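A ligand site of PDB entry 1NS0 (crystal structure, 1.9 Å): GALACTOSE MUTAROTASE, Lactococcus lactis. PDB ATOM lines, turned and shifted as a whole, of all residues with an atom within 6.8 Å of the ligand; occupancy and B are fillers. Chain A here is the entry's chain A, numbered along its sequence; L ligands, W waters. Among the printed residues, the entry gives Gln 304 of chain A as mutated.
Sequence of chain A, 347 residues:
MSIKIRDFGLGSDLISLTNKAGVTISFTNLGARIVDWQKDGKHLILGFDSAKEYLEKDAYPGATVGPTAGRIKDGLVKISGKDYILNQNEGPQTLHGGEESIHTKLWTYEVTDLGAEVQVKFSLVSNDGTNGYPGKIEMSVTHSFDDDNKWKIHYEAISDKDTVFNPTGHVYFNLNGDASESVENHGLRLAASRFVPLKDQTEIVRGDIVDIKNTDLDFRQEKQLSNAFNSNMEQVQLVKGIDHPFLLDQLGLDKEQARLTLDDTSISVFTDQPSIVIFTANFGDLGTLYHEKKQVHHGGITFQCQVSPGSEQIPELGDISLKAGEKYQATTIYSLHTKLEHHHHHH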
ATOM      1  N   ASP A  58       7.266  13.209  23.987  1.00  0.00           N
ATOM      2  CA  ASP A  58       7.258  13.463  22.559  1.00  0.00           C
ATOM      3  C   ASP A  58       6.973  14.925  22.443  1.00  0.00           C
ATOM      4  O   ASP A  58       5.933  15.354  22.932  1.00  0.00           O
ATOM      5  CB  ASP A  58       6.254  12.594  21.790  1.00  0.00           C
ATOM      6  CG  ASP A  58       6.287  12.886  20.307  1.00  0.00           C
ATOM      7  OD1 ASP A  58       7.053  13.682  19.800  1.00  0.00           O
ATOM      8  OD2 ASP A  58       5.467  12.152  19.583  1.00  0.00           O
ATOM      9  N   TYR A  60       6.542  16.722  19.687  1.00  0.00           N
ATOM     10  CA  TYR A  60       5.831  17.192  18.493  1.00  0.00           C
ATOM     11  C   TYR A  60       4.344  17.412  18.577  1.00  0.00           C
ATOM     12  O   TYR A  60       3.826  18.387  17.976  1.00  0.00           O
ATOM     13  CB  TYR A  60       6.149  16.265  17.305  1.00  0.00           C
ATOM     14  CG  TYR A  60       7.610  16.401  16.897  1.00  0.00           C
ATOM     15  CD1 TYR A  60       8.441  15.293  16.871  1.00  0.00           C
ATOM     16  CD2 TYR A  60       8.173  17.633  16.549  1.00  0.00           C
ATOM     17  CE1 TYR A  60       9.783  15.381  16.485  1.00  0.00           C
ATOM     18  CE2 TYR A  60       9.510  17.750  16.152  1.00  0.00           C
ATOM     19  CZ  TYR A  60      10.320  16.617  16.123  1.00  0.00           C
ATOM     20  OH  TYR A  60      11.639  16.704  15.736  1.00  0.00           O
ATOM     21  N   PRO A  61       3.659  16.515  19.296  1.00  0.00           N
ATOM     22  CA  PRO A  61       2.196  16.604  19.386  1.00  0.00           C
ATOM     23  C   PRO A  61       1.613  17.995  19.642  1.00  0.00           C
ATOM     24  O   PRO A  61       1.901  18.621  20.644  1.00  0.00           O
ATOM     25  CB  PRO A  61       1.745  15.578  20.422  1.00  0.00           C
ATOM     26  CG  PRO A  61       2.888  14.598  20.515  1.00  0.00           C
ATOM     27  CD  PRO A  61       4.147  15.338  20.077  1.00  0.00           C
ATOM     28  N   GLY A  70       8.730  18.768   8.190  1.00  0.00           N
ATOM     29  CA  GLY A  70       9.047  17.576   7.409  1.00  0.00           C
ATOM     30  C   GLY A  70      10.524  17.294   7.273  1.00  0.00           C
ATOM     31  O   GLY A  70      11.346  17.917   7.932  1.00  0.00           O
ATOM     32  N   ARG A  71      10.841  16.325   6.410  1.00  0.00           N
ATOM     33  CA  ARG A  71      12.214  15.933   6.181  1.00  0.00           C
ATOM     34  C   ARG A  71      12.840  16.577   4.975  1.00  0.00           C
ATOM     35  O   ARG A  71      12.257  16.577   3.855  1.00  0.00           O
ATOM     36  CB  ARG A  71      12.341  14.451   5.891  1.00  0.00           C
ATOM     37  CG  ARG A  71      11.757  13.635   7.003  1.00  0.00           C
ATOM     38  CD  ARG A  71      11.890  12.122   6.810  1.00  0.00           C
ATOM     39  NE  ARG A  71      11.642  11.530   8.156  1.00  0.00           N
ATOM     40  CZ  ARG A  71      10.444  11.349   8.744  1.00  0.00           C
ATOM     41  NH1 ARG A  71       9.235  11.556   8.153  1.00  0.00           N
ATOM     42  NH2 ARG A  71      10.479  10.856   9.963  1.00  0.00           N
ATOM     43  N   GLU A  90      18.111  13.536  12.156  1.00  0.00           N
ATOM     44  CA  GLU A  90      17.516  12.236  11.920  1.00  0.00           C
ATOM     45  C   GLU A  90      18.384  11.643  10.873  1.00  0.00           C
ATOM     46  O   GLU A  90      18.072  11.754   9.674  1.00  0.00           O
ATOM     47  CB  GLU A  90      16.155  12.398  11.284  1.00  0.00           C
ATOM     48  CG  GLU A  90      15.471  11.057  11.410  1.00  0.00           C
ATOM     49  CD  GLU A  90      14.192  10.993  10.606  1.00  0.00           C
ATOM     50  OE1 GLU A  90      14.153  11.313   9.451  1.00  0.00           O
ATOM     51  OE2 GLU A  90      13.140  10.571  11.269  1.00  0.00           O
ATOM     52  N   LEU A  95      14.877  16.980  10.145  1.00  0.00           N
ATOM     53  CA  LEU A  95      13.456  16.725  10.322  1.00  0.00           C
ATOM     54  C   LEU A  95      12.839  17.834  11.171  1.00  0.00           C
ATOM     55  O   LEU A  95      13.340  18.129  12.231  1.00  0.00           O
ATOM     56  CB  LEU A  95      13.248  15.360  11.016  1.00  0.00           C
ATOM     57  CG  LEU A  95      11.824  15.142  11.562  1.00  0.00           C
ATOM     58  CD1 LEU A  95      10.737  14.941  10.478  1.00  0.00           C
ATOM     59  CD2 LEU A  95      11.765  13.947  12.501  1.00  0.00           C
ATOM     60  N   HIS A  96      11.778  18.451  10.725  1.00  0.00           N
ATOM     61  CA  HIS A  96      11.143  19.517  11.525  1.00  0.00           C
ATOM     62  C   HIS A  96      12.071  20.621  12.044  1.00  0.00           C
ATOM     63  O   HIS A  96      11.972  21.031  13.211  1.00  0.00           O
ATOM     64  CB  HIS A  96      10.300  18.956  12.699  1.00  0.00           C
ATOM     65  CG  HIS A  96       9.214  18.024  12.257  1.00  0.00           C
ATOM     66  ND1 HIS A  96       8.514  18.204  11.054  1.00  0.00           N
ATOM     67  CD2 HIS A  96       8.719  16.932  12.889  1.00  0.00           C
ATOM     68  CE1 HIS A  96       7.631  17.220  10.984  1.00  0.00           C
ATOM     69  NE2 HIS A  96       7.723  16.448  12.063  1.00  0.00           N
ATOM     70  N   HIS A 170       1.227  20.434  14.155  1.00  0.00           N
ATOM     71  CA  HIS A 170       1.310  19.003  14.239  1.00  0.00           C
ATOM     72  C   HIS A 170       0.322  18.342  15.218  1.00  0.00           C
ATOM     73  O   HIS A 170       0.656  17.380  15.932  1.00  0.00           O
ATOM     74  CB  HIS A 170       2.757  18.649  14.609  1.00  0.00           C
ATOM     75  CG  HIS A 170       3.203  17.291  14.141  1.00  0.00           C
ATOM     76  ND1 HIS A 170       2.804  16.128  14.793  1.00  0.00           N
ATOM     77  CD2 HIS A 170       4.032  16.953  13.116  1.00  0.00           C
ATOM     78  CE1 HIS A 170       3.365  15.112  14.131  1.00  0.00           C
ATOM     79  NE2 HIS A 170       4.108  15.559  13.121  1.00  0.00           N
ATOM     80  N   TYR A 172      -2.552  15.936  16.545  1.00  0.00           N
ATOM     81  CA  TYR A 172      -2.977  14.577  16.254  1.00  0.00           C
ATOM     82  C   TYR A 172      -4.417  14.468  16.759  1.00  0.00           C
ATOM     83  O   TYR A 172      -4.730  14.766  17.924  1.00  0.00           O
ATOM     84  CB  TYR A 172      -2.240  13.527  17.087  1.00  0.00           C
ATOM     85  CG  TYR A 172      -0.829  13.180  16.640  1.00  0.00           C
ATOM     86  CD1 TYR A 172       0.278  13.839  17.195  1.00  0.00           C
ATOM     87  CD2 TYR A 172      -0.589  12.149  15.731  1.00  0.00           C
ATOM     88  CE1 TYR A 172       1.571  13.478  16.822  1.00  0.00           C
ATOM     89  CE2 TYR A 172       0.696  11.795  15.324  1.00  0.00           C
ATOM     90  CZ  TYR A 172       1.788  12.464  15.895  1.00  0.00           C
ATOM     91  OH  TYR A 172       3.072  12.102  15.533  1.00  0.00           O
ATOM     92  N   GLU A 203      12.374   7.616   4.729  1.00  0.00           N
ATOM     93  CA  GLU A 203      11.247   8.493   4.537  1.00  0.00           C
ATOM     94  C   GLU A 203      11.523   9.728   3.755  1.00  0.00           C
ATOM     95  O   GLU A 203      10.751  10.654   3.852  1.00  0.00           O
ATOM     96  CB  GLU A 203      10.398   8.757   5.801  1.00  0.00           C
ATOM     97  CG  GLU A 203       9.687   7.506   6.405  1.00  0.00           C
ATOM     98  CD  GLU A 203       9.474   7.420   7.929  1.00  0.00           C
ATOM     99  OE1 GLU A 203      10.350   7.308   8.776  1.00  0.00           O
ATOM    100  OE2 GLU A 203       8.208   7.384   8.247  1.00  0.00           O
ATOM    101  N   ASP A 243       2.019   7.991   5.988  1.00  0.00           N
ATOM    102  CA  ASP A 243       3.028   8.978   6.405  1.00  0.00           C
ATOM    103  C   ASP A 243       3.454   9.656   5.112  1.00  0.00           C
ATOM    104  O   ASP A 243       4.580   9.527   4.644  1.00  0.00           O
ATOM    105  CB  ASP A 243       4.185   8.306   7.186  1.00  0.00           C
ATOM    106  CG  ASP A 243       5.001   9.333   7.919  1.00  0.00           C
ATOM    107  OD1 ASP A 243       4.709  10.501   7.964  1.00  0.00           O
ATOM    108  OD2 ASP A 243       5.984   8.840   8.603  1.00  0.00           O
ATOM    109  N   HIS A 244       2.473  10.362   4.499  1.00  0.00           N
ATOM    110  CA  HIS A 244       2.660  10.951   3.204  1.00  0.00           C
ATOM    111  C   HIS A 244       1.932  12.244   2.933  1.00  0.00           C
ATOM    112  O   HIS A 244       0.833  12.447   3.460  1.00  0.00           O
ATOM    113  CB  HIS A 244       1.886   9.988   2.268  1.00  0.00           C
ATOM    114  CG  HIS A 244       2.583   8.669   2.120  1.00  0.00           C
ATOM    115  ND1 HIS A 244       2.366   7.616   3.029  1.00  0.00           N
ATOM    116  CD2 HIS A 244       3.486   8.296   1.175  1.00  0.00           C
ATOM    117  CE1 HIS A 244       3.153   6.629   2.636  1.00  0.00           C
ATOM    118  NE2 HIS A 244       3.809   6.997   1.522  1.00  0.00           N
ATOM    119  N   VAL A 277      -0.033  16.622   4.894  1.00  0.00           N
ATOM    120  CA  VAL A 277       0.718  15.443   5.263  1.00  0.00           C
ATOM    121  C   VAL A 277      -0.079  14.651   6.312  1.00  0.00           C
ATOM    122  O   VAL A 277      -0.429  15.150   7.389  1.00  0.00           O
ATOM    123  CB  VAL A 277       2.104  15.790   5.766  1.00  0.00           C
ATOM    124  CG1 VAL A 277       2.775  14.463   6.153  1.00  0.00           C
ATOM    125  CG2 VAL A 277       2.871  16.513   4.645  1.00  0.00           C
ATOM    126  N   ILE A 278      -0.381  13.394   5.979  1.00  0.00           N
ATOM    127  CA  ILE A 278      -1.151  12.548   6.857  1.00  0.00           C
ATOM    128  C   ILE A 278      -0.294  11.489   7.465  1.00  0.00           C
ATOM    129  O   ILE A 278       0.227  10.643   6.738  1.00  0.00           O
ATOM    130  CB  ILE A 278      -2.293  11.895   6.064  1.00  0.00           C
ATOM    131  CG1 ILE A 278      -3.188  13.048   5.622  1.00  0.00           C
ATOM    132  CG2 ILE A 278      -3.069  10.941   6.981  1.00  0.00           C
ATOM    133  CD1 ILE A 278      -4.467  12.630   4.970  1.00  0.00           C
ATOM    134  N   PHE A 279      -0.133  11.545   8.776  1.00  0.00           N
ATOM    135  CA  PHE A 279       0.693  10.541   9.447  1.00  0.00           C
ATOM    136  C   PHE A 279      -0.216   9.893  10.468  1.00  0.00           C
ATOM    137  O   PHE A 279      -0.867  10.608  11.237  1.00  0.00           O
ATOM    138  CB  PHE A 279       1.905  11.247  10.118  1.00  0.00           C
ATOM    139  CG  PHE A 279       2.679  10.428  11.113  1.00  0.00           C
ATOM    140  CD1 PHE A 279       3.252   9.215  10.705  1.00  0.00           C
ATOM    141  CD2 PHE A 279       2.842  10.877  12.429  1.00  0.00           C
ATOM    142  CE1 PHE A 279       4.006   8.449  11.584  1.00  0.00           C
ATOM    143  CE2 PHE A 279       3.555  10.107  13.328  1.00  0.00           C
ATOM    144  CZ  PHE A 279       4.163   8.926  12.889  1.00  0.00           C
ATOM    145  N   ASN A 282       2.214   5.692  13.440  1.00  0.00           N
ATOM    146  CA  ASN A 282       2.670   4.345  13.172  1.00  0.00           C
ATOM    147  C   ASN A 282       3.782   3.958  14.122  1.00  0.00           C
ATOM    148  O   ASN A 282       4.848   3.532  13.665  1.00  0.00           O
ATOM    149  CB  ASN A 282       3.147   4.287  11.704  1.00  0.00           C
ATOM    150  CG  ASN A 282       2.117   4.866  10.751  1.00  0.00           C
ATOM    151  OD1 ASN A 282       0.906   4.700  10.970  1.00  0.00           O
ATOM    152  ND2 ASN A 282       2.574   5.546   9.694  1.00  0.00           N
ATOM    153  N   PHE A 283       3.554   4.111  15.440  1.00  0.00           N
ATOM    154  CA  PHE A 283       4.591   3.840  16.451  1.00  0.00           C
ATOM    155  C   PHE A 283       4.779   2.402  16.948  1.00  0.00           C
ATOM    156  O   PHE A 283       5.535   2.155  17.902  1.00  0.00           O
ATOM    157  CB  PHE A 283       4.544   4.812  17.638  1.00  0.00           C
ATOM    158  CG  PHE A 283       4.460   6.269  17.224  1.00  0.00           C
ATOM    159  CD1 PHE A 283       3.293   7.020  17.417  1.00  0.00           C
ATOM    160  CD2 PHE A 283       5.566   6.923  16.670  1.00  0.00           C
ATOM    161  CE1 PHE A 283       3.220   8.359  17.059  1.00  0.00           C
ATOM    162  CE2 PHE A 283       5.511   8.272  16.309  1.00  0.00           C
ATOM    163  CZ  PHE A 283       4.327   8.985  16.494  1.00  0.00           C
ATOM    164  N   THR A 302      -2.656  12.992  11.829  1.00  0.00           N
ATOM    165  CA  THR A 302      -2.370  14.399  11.615  1.00  0.00           C
ATOM    166  C   THR A 302      -2.956  14.882  10.306  1.00  0.00           C
ATOM    167  O   THR A 302      -3.206  14.096   9.397  1.00  0.00           O
ATOM    168  CB  THR A 302      -0.820  14.657  11.476  1.00  0.00           C
ATOM    169  OG1 THR A 302      -0.341  14.070  10.268  1.00  0.00           O
ATOM    170  CG2 THR A 302       0.052  14.221  12.645  1.00  0.00           C
ATOM    171  N   GLN A 304      -1.219  17.787   8.530  1.00  0.00           N
ATOM    172  CA  GLN A 304      -0.251  18.875   8.524  1.00  0.00           C
ATOM    173  C   GLN A 304      -0.352  19.628   7.227  1.00  0.00           C
ATOM    174  O   GLN A 304       0.084  19.150   6.200  1.00  0.00           O
ATOM    175  CB  GLN A 304       1.191  18.329   8.633  1.00  0.00           C
ATOM    176  CG  GLN A 304       1.336  17.434   9.878  1.00  0.00           C
ATOM    177  CD  GLN A 304       2.577  16.567   9.870  1.00  0.00           C
ATOM    178  OE1 GLN A 304       2.489  15.321   9.898  1.00  0.00           O
ATOM    179  NE2 GLN A 304       3.743  17.202   9.850  1.00  0.00           N
HETATM  180  C1  LIG L   1       5.805  13.698  11.008  1.00  0.00           C
HETATM  181  C2  LIG L   1       6.522  12.621  10.184  1.00  0.00           C
HETATM  182  C3  LIG L   1       6.438  11.280  10.887  1.00  0.00           C
HETATM  183  C4  LIG L   1       7.100  11.412  12.251  1.00  0.00           C
HETATM  184  C5  LIG L   1       6.482  12.593  13.041  1.00  0.00           C
HETATM  185  C6  LIG L   1       7.217  12.982  14.336  1.00  0.00           C
HETATM  186  O1  LIG L   1       4.390  13.567  11.117  1.00  0.00           O
HETATM  187  O2  LIG L   1       6.085  12.436   8.852  1.00  0.00           O
HETATM  188  O3  LIG L   1       7.219  10.358  10.117  1.00  0.00           O
HETATM  189  O4  LIG L   1       8.501  11.599  12.088  1.00  0.00           O
HETATM  190  O5  LIG L   1       6.463  13.807  12.262  1.00  0.00           O
HETATM  191  O6  LIG L   1       6.753  12.217  15.436  1.00  0.00           O
HETATM  192  O   HOH W   1       6.534  14.725   7.105  1.00  0.00           O
HETATM  193  O   HOH W   2       5.049  12.875  17.170  1.00  0.00           O
HETATM  194  O   HOH W   3       8.153   8.010  11.385  1.00  0.00           O
HETATM  195  O   HOH W   4       9.770  10.900  14.261  1.00  0.00           O
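Tyr 60 touches the ligand.
OH of Tyr 172 touches O6 of the ligand, 3.7 Å away.
Glu 203 touches the ligand.
Phe 279 touches the ligand.
Of the 20 residues printed, 9 come within 4 Å of the ligand.
The nearest printed residue that does not touch the ligand is Leu 95 (4.04 Å).
NE2 of His 96 sits at hydrogen-bond distance from O5 of the ligand (2.9 Å).
O1 of the ligand is in hydrogen-bond range of OE1 of Gln 304, at 2.9 Å.
An oxygen (O3) of the ligand is in hydrogen-bond range of the side-chain carboxylate (OD2) of Asp 243, 2.5 Å away.
NE2 of His 170 is in hydrogen-bond range of O1 of the ligand (2.8 Å).
The guanidinium group (NH2) of Arg 71 is in hydrogen-bond range of an oxygen (O4) of the ligand (3.0 Å).
N of Tyr 60 is in hydrogen-bond range of OD1 of Asp 58.
The guanidinium group of Arg 71 is in salt-bridge range of the side-chain carboxylate of Glu 203, at 3.7 Å.
The backbone NH of Phe 279 lies within hydrogen-bond range of the side-chain hydroxyl of Thr 302, 2.9 Å away.
The side-chain carboxylate of Asp 243 lies close to the side-chain carboxylate of Glu 203 (2.7 Å).
The guanidinium group (NE) of Arg 71 is in salt-bridge range of the side-chain carboxylate (OE1) of Glu 90 (2.8 Å).
The side-chain amide oxygen (OE1) of Gln 304 lies within hydrogen-bond range of the side-chain hydroxyl (OG1) of Thr 302 (3.1 Å).
The backbone carbonyl oxygen (O) of Gly 70 is in hydrogen-bond range of the backbone NH (N) of His 96 (2.9 Å).
N of Asp 243 lies close to O of Ile 278.
Water W2 lies within hydrogen-bond range of an oxygen (O6) of the ligand (2.5 Å), the side-chain carboxylate of Asp 58 (2.6 Å) and the side-chain hydroxyl of Tyr 172 (2.7 Å).
Water W3 lies within hydrogen-bond range of O3 of the ligand (2.8 Å) and OE2 of Glu 203 (3.2 Å).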
